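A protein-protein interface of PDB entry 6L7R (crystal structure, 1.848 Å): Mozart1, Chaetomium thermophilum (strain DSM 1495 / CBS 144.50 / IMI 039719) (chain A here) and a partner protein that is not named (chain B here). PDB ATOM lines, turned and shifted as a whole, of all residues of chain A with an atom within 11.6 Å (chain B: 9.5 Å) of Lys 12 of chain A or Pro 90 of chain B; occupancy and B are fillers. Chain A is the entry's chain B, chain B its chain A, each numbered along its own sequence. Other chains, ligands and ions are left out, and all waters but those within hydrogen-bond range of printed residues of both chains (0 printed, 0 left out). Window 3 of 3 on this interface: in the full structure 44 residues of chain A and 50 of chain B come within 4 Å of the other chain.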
ATOM      1  N   MET A   4      22.313 -13.019   9.712  1.00  0.00           N
ATOM      2  CA  MET A   4      22.557 -12.712   8.304  1.00  0.00           C
ATOM      3  C   MET A   4      23.745 -11.728   8.211  1.00  0.00           C
ATOM      4  O   MET A   4      23.739 -10.673   8.848  1.00  0.00           O
ATOM      5  CB  MET A   4      21.253 -12.185   7.659  1.00  0.00           C
ATOM      6  CG  MET A   4      21.361 -11.471   6.320  1.00  0.00           C
ATOM      7  SD  MET A   4      19.777 -10.985   5.561  1.00  0.00           S
ATOM      8  CE  MET A   4      18.831 -12.496   5.629  1.00  0.00           C
ATOM      9  N   PRO A   5      24.783 -12.087   7.456  1.00  0.00           N
ATOM     10  CA  PRO A   5      26.000 -11.249   7.410  1.00  0.00           C
ATOM     11  C   PRO A   5      25.762  -9.975   6.615  1.00  0.00           C
ATOM     12  O   PRO A   5      24.802  -9.898   5.837  1.00  0.00           O
ATOM     13  CB  PRO A   5      27.028 -12.156   6.714  1.00  0.00           C
ATOM     14  CG  PRO A   5      26.213 -13.071   5.879  1.00  0.00           C
ATOM     15  CD  PRO A   5      24.928 -13.311   6.649  1.00  0.00           C
ATOM     16  N   PRO A   6      26.626  -8.962   6.772  1.00  0.00           N
ATOM     17  CA  PRO A   6      26.416  -7.690   6.045  1.00  0.00           C
ATOM     18  C   PRO A   6      26.187  -7.829   4.544  1.00  0.00           C
ATOM     19  O   PRO A   6      25.339  -7.119   3.983  1.00  0.00           O
ATOM     20  CB  PRO A   6      27.708  -6.921   6.344  1.00  0.00           C
ATOM     21  CG  PRO A   6      28.097  -7.393   7.710  1.00  0.00           C
ATOM     22  CD  PRO A   6      27.697  -8.850   7.778  1.00  0.00           C
ATOM     23  N   SER A   7      26.925  -8.716   3.874  1.00  0.00           N
ATOM     24  CA  SER A   7      26.783  -8.831   2.428  1.00  0.00           C
ATOM     25  C   SER A   7      25.373  -9.253   2.047  1.00  0.00           C
ATOM     26  O   SER A   7      24.801  -8.731   1.089  1.00  0.00           O
ATOM     27  CB  SER A   7      27.801  -9.822   1.875  1.00  0.00           C
ATOM     28  OG  SER A   7      27.681 -11.068   2.535  1.00  0.00           O
ATOM     29  N   GLU A   8      24.793 -10.193   2.792  1.00  0.00           N
ATOM     30  CA  GLU A   8      23.456 -10.668   2.453  1.00  0.00           C
ATOM     31  C   GLU A   8      22.395  -9.629   2.793  1.00  0.00           C
ATOM     32  O   GLU A   8      21.412  -9.475   2.058  1.00  0.00           O
ATOM     33  CB  GLU A   8      23.171 -11.983   3.176  1.00  0.00           C
ATOM     34  CG  GLU A   8      21.867 -12.644   2.759  1.00  0.00           C
ATOM     35  CD  GLU A   8      21.632 -13.964   3.475  1.00  0.00           C
ATOM     36  OE1 GLU A   8      22.557 -14.445   4.173  1.00  0.00           O
ATOM     37  OE2 GLU A   8      20.526 -14.524   3.323  1.00  0.00           O
ATOM     38  N   ARG A   9      22.569  -8.911   3.906  1.00  0.00           N
ATOM     39  CA  ARG A   9      21.640  -7.833   4.237  1.00  0.00           C
ATOM     40  C   ARG A   9      21.645  -6.751   3.164  1.00  0.00           C
ATOM     41  O   ARG A   9      20.580  -6.254   2.765  1.00  0.00           O
ATOM     42  CB  ARG A   9      21.992  -7.219   5.589  1.00  0.00           C
ATOM     43  CG  ARG A   9      21.736  -8.110   6.791  1.00  0.00           C
ATOM     44  CD  ARG A   9      21.817  -7.324   8.100  1.00  0.00           C
ATOM     45  NE  ARG A   9      21.381  -5.936   7.945  1.00  0.00           N
ATOM     46  CZ  ARG A   9      20.164  -5.483   8.231  1.00  0.00           C
ATOM     47  NH1 ARG A   9      19.227  -6.306   8.683  1.00  0.00           N
ATOM     48  NH2 ARG A   9      19.883  -4.198   8.059  1.00  0.00           N
ATOM     49  N   ALA A  10      22.838  -6.364   2.697  1.00  0.00           N
ATOM     50  CA  ALA A  10      22.950  -5.353   1.649  1.00  0.00           C
ATOM     51  C   ALA A  10      22.334  -5.840   0.344  1.00  0.00           C
ATOM     52  O   ALA A  10      21.625  -5.086  -0.336  1.00  0.00           O
ATOM     53  CB  ALA A  10      24.418  -4.967   1.439  1.00  0.00           C
ATOM     54  N   GLU A  11      22.611  -7.092  -0.037  1.00  0.00           N
ATOM     55  CA  GLU A  11      22.006  -7.639  -1.250  1.00  0.00           C
ATOM     56  C   GLU A  11      20.488  -7.684  -1.143  1.00  0.00           C
ATOM     57  O   GLU A  11      19.780  -7.367  -2.106  1.00  0.00           O
ATOM     58  CB  GLU A  11      22.560  -9.036  -1.538  1.00  0.00           C
ATOM     59  CG  GLU A  11      24.036  -9.034  -1.890  1.00  0.00           C
ATOM     60  CD  GLU A  11      24.601 -10.437  -1.986  1.00  0.00           C
ATOM     61  OE1 GLU A  11      23.872 -11.402  -1.663  1.00  0.00           O
ATOM     62  OE2 GLU A  11      25.771 -10.569  -2.392  1.00  0.00           O
ATOM     63  N   LYS A  12      19.963  -8.070   0.022  1.00  0.00           N
ATOM     64  CA  LYS A  12      18.513  -8.131   0.159  1.00  0.00           C
ATOM     65  C   LYS A  12      17.888  -6.745   0.162  1.00  0.00           C
ATOM     66  O   LYS A  12      16.788  -6.562  -0.369  1.00  0.00           O
ATOM     67  CB  LYS A  12      18.128  -8.901   1.424  1.00  0.00           C
ATOM     68  CG  LYS A  12      18.271 -10.407   1.267  1.00  0.00           C
ATOM     69  CD  LYS A  12      17.380 -11.177   2.231  1.00  0.00           C
ATOM     70  CE  LYS A  12      17.254 -12.639   1.811  1.00  0.00           C
ATOM     71  NZ  LYS A  12      18.537 -13.383   1.960  1.00  0.00           N
ATOM     72  N   GLN A  13      18.571  -5.749   0.728  1.00  0.00           N
ATOM     73  CA  GLN A  13      18.024  -4.399   0.681  1.00  0.00           C
ATOM     74  C   GLN A  13      18.023  -3.860  -0.743  1.00  0.00           C
ATOM     75  O   GLN A  13      17.069  -3.185  -1.158  1.00  0.00           O
ATOM     76  CB  GLN A  13      18.812  -3.470   1.598  1.00  0.00           C
ATOM     77  CG  GLN A  13      18.306  -2.048   1.561  1.00  0.00           C
ATOM     78  CD  GLN A  13      19.267  -1.100   2.224  1.00  0.00           C
ATOM     79  OE1 GLN A  13      20.040  -1.505   3.094  1.00  0.00           O
ATOM     80  NE2 GLN A  13      19.238   0.165   1.814  1.00  0.00           N
ATOM     81  N   ALA A  14      19.084  -4.147  -1.503  1.00  0.00           N
ATOM     82  CA  ALA A  14      19.129  -3.728  -2.903  1.00  0.00           C
ATOM     83  C   ALA A  14      18.065  -4.443  -3.727  1.00  0.00           C
ATOM     84  O   ALA A  14      17.432  -3.832  -4.591  1.00  0.00           O
ATOM     85  CB  ALA A  14      20.520  -3.978  -3.488  1.00  0.00           C
ATOM     86  N   ALA A  15      17.851  -5.737  -3.470  1.00  0.00           N
ATOM     87  CA  ALA A  15      16.810  -6.474  -4.184  1.00  0.00           C
ATOM     88  C   ALA A  15      15.413  -5.990  -3.810  1.00  0.00           C
ATOM     89  O   ALA A  15      14.514  -5.990  -4.661  1.00  0.00           O
ATOM     90  CB  ALA A  15      16.941  -7.972  -3.913  1.00  0.00           C
ATOM     91  N   ALA A  16      15.202  -5.586  -2.551  1.00  0.00           N
ATOM     92  CA  ALA A  16      13.908  -5.021  -2.171  1.00  0.00           C
ATOM     93  C   ALA A  16      13.582  -3.782  -2.997  1.00  0.00           C
ATOM     94  O   ALA A  16      12.427  -3.578  -3.404  1.00  0.00           O
ATOM     95  CB  ALA A  16      13.891  -4.682  -0.678  1.00  0.00           C
ATOM     96  N   GLN A  17      14.581  -2.930  -3.229  1.00  0.00           N
ATOM     97  CA  GLN A  17      14.350  -1.730  -4.026  1.00  0.00           C
ATOM     98  C   GLN A  17      14.035  -2.082  -5.476  1.00  0.00           C
ATOM     99  O   GLN A  17      13.152  -1.466  -6.091  1.00  0.00           O
ATOM    100  CB  GLN A  17      15.561  -0.800  -3.941  1.00  0.00           C
ATOM    101  CG  GLN A  17      15.567   0.276  -5.014  1.00  0.00           C
ATOM    102  CD  GLN A  17      16.472   1.455  -4.671  1.00  0.00           C
ATOM    103  OE1 GLN A  17      17.348   1.350  -3.819  1.00  0.00           O
ATOM    104  NE2 GLN A  17      16.260   2.580  -5.342  1.00  0.00           N
ATOM    105  N   GLN A  18      14.748  -3.065  -6.043  1.00  0.00           N
ATOM    106  CA  GLN A  18      14.418  -3.540  -7.385  1.00  0.00           C
ATOM    107  C   GLN A  18      13.008  -4.129  -7.433  1.00  0.00           C
ATOM    108  O   GLN A  18      12.297  -3.972  -8.432  1.00  0.00           O
ATOM    109  CB  GLN A  18      15.444  -4.575  -7.845  1.00  0.00           C
ATOM    110  CG  GLN A  18      16.812  -3.986  -8.092  1.00  0.00           C
ATOM    111  CD  GLN A  18      16.758  -2.840  -9.079  1.00  0.00           C
ATOM    112  OE1 GLN A  18      16.226  -2.983 -10.183  1.00  0.00           O
ATOM    113  NE2 GLN A  18      17.287  -1.687  -8.679  1.00  0.00           N
ATOM    114  N   ALA A  19      12.593  -4.818  -6.371  1.00  0.00           N
ATOM    115  CA  ALA A  19      11.240  -5.369  -6.327  1.00  0.00           C
ATOM    116  C   ALA A  19      10.189  -4.270  -6.440  1.00  0.00           C
ATOM    117  O   ALA A  19       9.203  -4.420  -7.174  1.00  0.00           O
ATOM    118  CB  ALA A  19      11.037  -6.182  -5.041  1.00  0.00           C
ATOM    119  N   VAL A  20      10.376  -3.159  -5.724  1.00  0.00           N
ATOM    120  CA  VAL A  20       9.422  -2.053  -5.826  1.00  0.00           C
ATOM    121  C   VAL A  20       9.444  -1.460  -7.234  1.00  0.00           C
ATOM    122  O   VAL A  20       8.390  -1.176  -7.818  1.00  0.00           O
ATOM    123  CB  VAL A  20       9.703  -0.982  -4.755  1.00  0.00           C
ATOM    124  CG1 VAL A  20       8.724   0.185  -4.891  1.00  0.00           C
ATOM    125  CG2 VAL A  20       9.630  -1.591  -3.353  1.00  0.00           C
ATOM    126  N   ASP A  21      10.639  -1.269  -7.803  1.00  0.00           N
ATOM    127  CA  ASP A  21      10.741  -0.750  -9.166  1.00  0.00           C
ATOM    128  C   ASP A  21      10.009  -1.647 -10.153  1.00  0.00           C
ATOM    129  O   ASP A  21       9.286  -1.166 -11.033  1.00  0.00           O
ATOM    130  CB  ASP A  21      12.208  -0.631  -9.589  1.00  0.00           C
ATOM    131  CG  ASP A  21      12.959   0.462  -8.848  1.00  0.00           C
ATOM    132  OD1 ASP A  21      12.339   1.213  -8.060  1.00  0.00           O
ATOM    133  OD2 ASP A  21      14.183   0.573  -9.077  1.00  0.00           O
ATOM    134  N   ILE A  22      10.222  -2.962 -10.047  1.00  0.00           N
ATOM    135  CA  ILE A  22       9.579  -3.893 -10.969  1.00  0.00           C
ATOM    136  C   ILE A  22       8.071  -3.890 -10.758  1.00  0.00           C
ATOM    137  O   ILE A  22       7.292  -3.817 -11.716  1.00  0.00           O
ATOM    138  CB  ILE A  22      10.159  -5.304 -10.797  1.00  0.00           C
ATOM    139  CG1 ILE A  22      11.618  -5.352 -11.269  1.00  0.00           C
ATOM    140  CG2 ILE A  22       9.311  -6.327 -11.539  1.00  0.00           C
ATOM    141  CD1 ILE A  22      12.316  -6.633 -10.840  1.00  0.00           C
ATOM    142  N   LEU A  23       7.640  -3.989  -9.500  1.00  0.00           N
ATOM    143  CA  LEU A  23       6.216  -4.072  -9.229  1.00  0.00           C
ATOM    144  C   LEU A  23       5.504  -2.768  -9.554  1.00  0.00           C
ATOM    145  O   LEU A  23       4.346  -2.793  -9.975  1.00  0.00           O
ATOM    146  CB  LEU A  23       5.981  -4.484  -7.767  1.00  0.00           C
ATOM    147  CG  LEU A  23       6.248  -5.956  -7.458  1.00  0.00           C
ATOM    148  CD1 LEU A  23       6.551  -6.184  -5.966  1.00  0.00           C
ATOM    149  CD2 LEU A  23       5.056  -6.789  -7.921  1.00  0.00           C
ATOM    150  N   ILE A  43       2.875  -3.807  -0.105  1.00  0.00           N
ATOM    151  CA  ILE A  43       3.895  -4.858  -0.039  1.00  0.00           C
ATOM    152  C   ILE A  43       4.158  -5.240   1.415  1.00  0.00           C
ATOM    153  O   ILE A  43       4.179  -6.425   1.779  1.00  0.00           O
ATOM    154  CB  ILE A  43       5.180  -4.398  -0.755  1.00  0.00           C
ATOM    155  CG1 ILE A  43       4.949  -4.288  -2.258  1.00  0.00           C
ATOM    156  CG2 ILE A  43       6.344  -5.352  -0.470  1.00  0.00           C
ATOM    157  CD1 ILE A  43       6.083  -3.589  -3.009  1.00  0.00           C
ATOM    158  N   GLU A  47       3.430  -8.896   2.955  1.00  0.00           N
ATOM    159  CA  GLU A  47       4.544  -9.675   3.493  1.00  0.00           C
ATOM    160  C   GLU A  47       4.338 -10.001   4.970  1.00  0.00           C
ATOM    161  O   GLU A  47       4.959 -10.942   5.485  1.00  0.00           O
ATOM    162  CB  GLU A  47       5.857  -8.922   3.279  1.00  0.00           C
ATOM    163  CG  GLU A  47       6.308  -8.913   1.813  1.00  0.00           C
ATOM    164  CD  GLU A  47       6.585 -10.330   1.291  1.00  0.00           C
ATOM    165  OE1 GLU A  47       7.311 -11.075   1.983  1.00  0.00           O
ATOM    166  OE2 GLU A  47       6.070 -10.705   0.206  1.00  0.00           O
ATOM    167  N   THR B  84       9.384 -12.428 -14.866  1.00  0.00           N
ATOM    168  CA  THR B  84      10.526 -13.320 -14.735  1.00  0.00           C
ATOM    169  C   THR B  84      11.590 -12.716 -13.829  1.00  0.00           C
ATOM    170  O   THR B  84      12.149 -13.405 -12.967  1.00  0.00           O
ATOM    171  CB  THR B  84      11.098 -13.626 -16.115  1.00  0.00           C
ATOM    172  OG1 THR B  84      10.152 -14.404 -16.856  1.00  0.00           O
ATOM    173  CG2 THR B  84      12.404 -14.393 -15.996  1.00  0.00           C
ATOM    174  N   ARG B  85      11.897 -11.427 -14.024  1.00  0.00           N
ATOM    175  CA  ARG B  85      12.873 -10.755 -13.171  1.00  0.00           C
ATOM    176  C   ARG B  85      12.445 -10.821 -11.718  1.00  0.00           C
ATOM    177  O   ARG B  85      13.250 -11.115 -10.827  1.00  0.00           O
ATOM    178  CB  ARG B  85      13.036  -9.293 -13.582  1.00  0.00           C
ATOM    179  CG  ARG B  85      13.750  -9.047 -14.902  1.00  0.00           C
ATOM    180  CD  ARG B  85      14.008  -7.526 -15.043  1.00  0.00           C
ATOM    181  NE  ARG B  85      14.659  -6.994 -13.847  1.00  0.00           N
ATOM    182  CZ  ARG B  85      14.697  -5.705 -13.521  1.00  0.00           C
ATOM    183  NH1 ARG B  85      14.093  -4.801 -14.276  1.00  0.00           N
ATOM    184  NH2 ARG B  85      15.331  -5.322 -12.421  1.00  0.00           N
ATOM    185  N   LEU B  86      11.173 -10.530 -11.467  1.00  0.00           N
ATOM    186  CA  LEU B  86      10.680 -10.503 -10.094  1.00  0.00           C
ATOM    187  C   LEU B  86      10.869 -11.851  -9.416  1.00  0.00           C
ATOM    188  O   LEU B  86      11.300 -11.918  -8.259  1.00  0.00           O
ATOM    189  CB  LEU B  86       9.207 -10.106 -10.090  1.00  0.00           C
ATOM    190  CG  LEU B  86       8.551 -10.125  -8.714  1.00  0.00           C
ATOM    191  CD1 LEU B  86       9.116  -9.008  -7.864  1.00  0.00           C
ATOM    192  CD2 LEU B  86       7.036 -10.010  -8.848  1.00  0.00           C
ATOM    193  N   LEU B  87      10.548 -12.937 -10.120  1.00  0.00           N
ATOM    194  CA  LEU B  87      10.620 -14.264  -9.516  1.00  0.00           C
ATOM    195  C   LEU B  87      12.033 -14.603  -9.061  1.00  0.00           C
ATOM    196  O   LEU B  87      12.208 -15.349  -8.090  1.00  0.00           O
ATOM    197  CB  LEU B  87      10.136 -15.321 -10.507  1.00  0.00           C
ATOM    198  CG  LEU B  87       8.677 -15.322 -10.949  1.00  0.00           C
ATOM    199  CD1 LEU B  87       8.428 -16.562 -11.784  1.00  0.00           C
ATOM    200  CD2 LEU B  87       7.762 -15.282  -9.747  1.00  0.00           C
ATOM    201  N   ALA B  88      13.047 -14.077  -9.751  1.00  0.00           N
ATOM    202  CA  ALA B  88      14.440 -14.394  -9.454  1.00  0.00           C
ATOM    203  C   ALA B  88      14.994 -13.623  -8.259  1.00  0.00           C
ATOM    204  O   ALA B  88      16.073 -13.970  -7.765  1.00  0.00           O
ATOM    205  CB  ALA B  88      15.312 -14.125 -10.688  1.00  0.00           C
ATOM    206  N   LEU B  89      14.299 -12.597  -7.785  1.00  0.00           N
ATOM    207  CA  LEU B  89      14.844 -11.770  -6.717  1.00  0.00           C
ATOM    208  C   LEU B  89      14.857 -12.550  -5.405  1.00  0.00           C
ATOM    209  O   LEU B  89      13.942 -13.339  -5.142  1.00  0.00           O
ATOM    210  CB  LEU B  89      14.027 -10.486  -6.558  1.00  0.00           C
ATOM    211  CG  LEU B  89      14.097  -9.456  -7.692  1.00  0.00           C
ATOM    212  CD1 LEU B  89      13.188  -8.273  -7.384  1.00  0.00           C
ATOM    213  CD2 LEU B  89      15.529  -8.983  -7.943  1.00  0.00           C
ATOM    214  N   PRO B  90      15.890 -12.361  -4.560  1.00  0.00           N
ATOM    215  CA  PRO B  90      15.982 -13.124  -3.306  1.00  0.00           C
ATOM    216  C   PRO B  90      15.210 -12.488  -2.165  1.00  0.00           C
ATOM    217  O   PRO B  90      15.579 -12.626  -0.997  1.00  0.00           O
ATOM    218  CB  PRO B  90      17.484 -13.108  -3.013  1.00  0.00           C
ATOM    219  CG  PRO B  90      17.916 -11.770  -3.531  1.00  0.00           C
ATOM    220  CD  PRO B  90      17.104 -11.557  -4.798  1.00  0.00           C
ATOM    221  N   VAL B  91      14.132 -11.787  -2.492  1.00  0.00           N
ATOM    222  CA  VAL B  91      13.360 -11.045  -1.509  1.00  0.00           C
ATOM    223  C   VAL B  91      11.888 -11.311  -1.801  1.00  0.00           C
ATOM    224  O   VAL B  91      11.521 -11.748  -2.894  1.00  0.00           O
ATOM    225  CB  VAL B  91      13.726  -9.538  -1.571  1.00  0.00           C
ATOM    226  CG1 VAL B  91      13.318  -8.931  -2.928  1.00  0.00           C
ATOM    227  CG2 VAL B  91      13.144  -8.755  -0.408  1.00  0.00           C
ATOM    228  N   LEU B  92      11.051 -11.073  -0.787  1.00  0.00           N
ATOM    229  CA  LEU B  92       9.600 -11.205  -0.858  1.00  0.00           C
ATOM    230  C   LEU B  92       9.155 -12.663  -0.844  1.00  0.00           C
ATOM    231  O   LEU B  92       9.428 -13.412  -1.787  1.00  0.00           O
ATOM    232  CB  LEU B  92       9.027 -10.490  -2.090  1.00  0.00           C
ATOM    233  CG  LEU B  92       9.270  -8.978  -2.212  1.00  0.00           C
ATOM    234  CD1 LEU B  92       8.605  -8.457  -3.482  1.00  0.00           C
ATOM    235  CD2 LEU B  92       8.755  -8.234  -0.972  1.00  0.00           C
ATOM    236  N   ASN B  93       8.448 -13.060   0.224  1.00  0.00           N
ATOM    237  CA  ASN B  93       7.937 -14.414   0.380  1.00  0.00           C
ATOM    238  C   ASN B  93       6.543 -14.603  -0.201  1.00  0.00           C
ATOM    239  O   ASN B  93       6.086 -15.748  -0.309  1.00  0.00           O
ATOM    240  CB  ASN B  93       7.910 -14.805   1.872  1.00  0.00           C
ATOM    241  CG  ASN B  93       9.248 -14.581   2.555  1.00  0.00           C
ATOM    242  OD1 ASN B  93       9.360 -13.806   3.508  1.00  0.00           O
ATOM    243  ND2 ASN B  93      10.277 -15.245   2.054  1.00  0.00           N
ATOM    244  N   LYS B  95       5.156 -13.300  -3.321  1.00  0.00           N
ATOM    245  CA  LYS B  95       5.089 -12.667  -4.634  1.00  0.00           C
ATOM    246  C   LYS B  95       3.741 -12.913  -5.297  1.00  0.00           C
ATOM    247  O   LYS B  95       3.180 -12.008  -5.928  1.00  0.00           O
ATOM    248  CB  LYS B  95       6.239 -13.174  -5.520  1.00  0.00           C
ATOM    249  CG  LYS B  95       7.601 -12.720  -5.041  1.00  0.00           C
ATOM    250  CD  LYS B  95       8.702 -13.174  -5.999  1.00  0.00           C
ATOM    251  CE  LYS B  95      10.087 -12.804  -5.492  1.00  0.00           C
ATOM    252  NZ  LYS B  95      10.538 -13.713  -4.401  1.00  0.00           N
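The side-chain amide oxygen (OE1) of Gln 18 of chain A sits at hydrogen-bond distance from the guanidinium group (NH2) of Arg 85 of chain B, at 3.4 Å.
The backbone NH (N) of Asn 93 of chain B sits at hydrogen-bond distance from the side-chain carboxylate (OE1) of Glu 47 of chain A, 2.9 Å away.
The side-chain amino group (NZ) of Lys 95 of chain B lies within hydrogen-bond range of the backbone carbonyl oxygen (O) of Val 91 of chain B, 2.7 Å away.
The side-chain amino group of Lys 95 of chain B lies within hydrogen-bond range of the backbone carbonyl oxygen of Leu 92 of chain B.
The side-chain carboxylate of Glu 8 of chain A is in salt-bridge range of the side-chain amino group of Lys 12 of chain A (2.7 Å).
Among the printed residues, pairs that only touch across the chains: Lys 12 of chain A with Pro 90 of chain B (3.3 Å), Ala 15 of chain A with Val 91 of chain B (3.6 Å), Ile 22 of chain A with Arg 85 of chain B (3.6 Å), Ala 19 of chain A with Leu 89 of chain B (3.6 Å), Glu 47 of chain A with Leu 92 of chain B (3.7 Å), Ala 19 of chain A with Leu 92 of chain B (3.7 Å), Ala 15 of chain A with Pro 90 of chain B (3.7 Å), Ile 43 of chain A with Leu 92 of chain B (3.8 Å), Ala 15 of chain A with Leu 89 of chain B (3.8 Å), Ala 16 of chain A with Val 91 of chain B (3.9 Å), Leu 23 of chain A with Leu 86 of chain B (3.9 Å), Ile 22 of chain A with Leu 89 of chain B (3.9 Å) and Leu 23 of chain A with Leu 92 of chain B (3.9 Å).
Ala 10 of chain A touches none of the printed residues of chain B.
Lys 12 of chain A touches one residue of chain B.
No residue of chain B comes within 4 Å of Ala 14 of chain A.
Ala 15 of chain A touches three residues of chain B.
Of the printed residues of chain B, Leu 23 of chain A touches Leu 86 (3.9 Å) and Leu 92 (3.9 Å).
Printed residues of chain B within 4 Å of Ile 43 of chain A: Leu 92 (3.8 Å).
Printed residues of chain B within 4 Å of Glu 47 of chain A: Leu 92 and Asn 93.
Of the printed residues of chain A, Pro 90 of chain B touches Lys 12 and Ala 15.
Of the printed residues of chain A, Leu 92 of chain B touches Ala 19, Leu 23, Ile 43 and Glu 47.
Of the printed residues of chain A, Asn 93 of chain B touches Glu 47.
The nearest residue of chain A that does not touch Pro 90 of chain B is Glu 11 of chain A (5.0 Å).
The nearest printed residue of chain A that does not touch Leu 86 of chain B is Ile 22 of chain A (4.05 Å).
Of the 11 printed residues of chain B, 7 touch a printed residue of chain A.
Hydrophobic or aromatic side chains of chain B that line the printed part of chain A: Leu 86, Leu 89, Pro 90, Val 91 and Leu 92.
Among the printed residues, no Asp or Glu carboxylate lies within 4 Å of a Lys or Arg side-chain nitrogen of the other chain.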
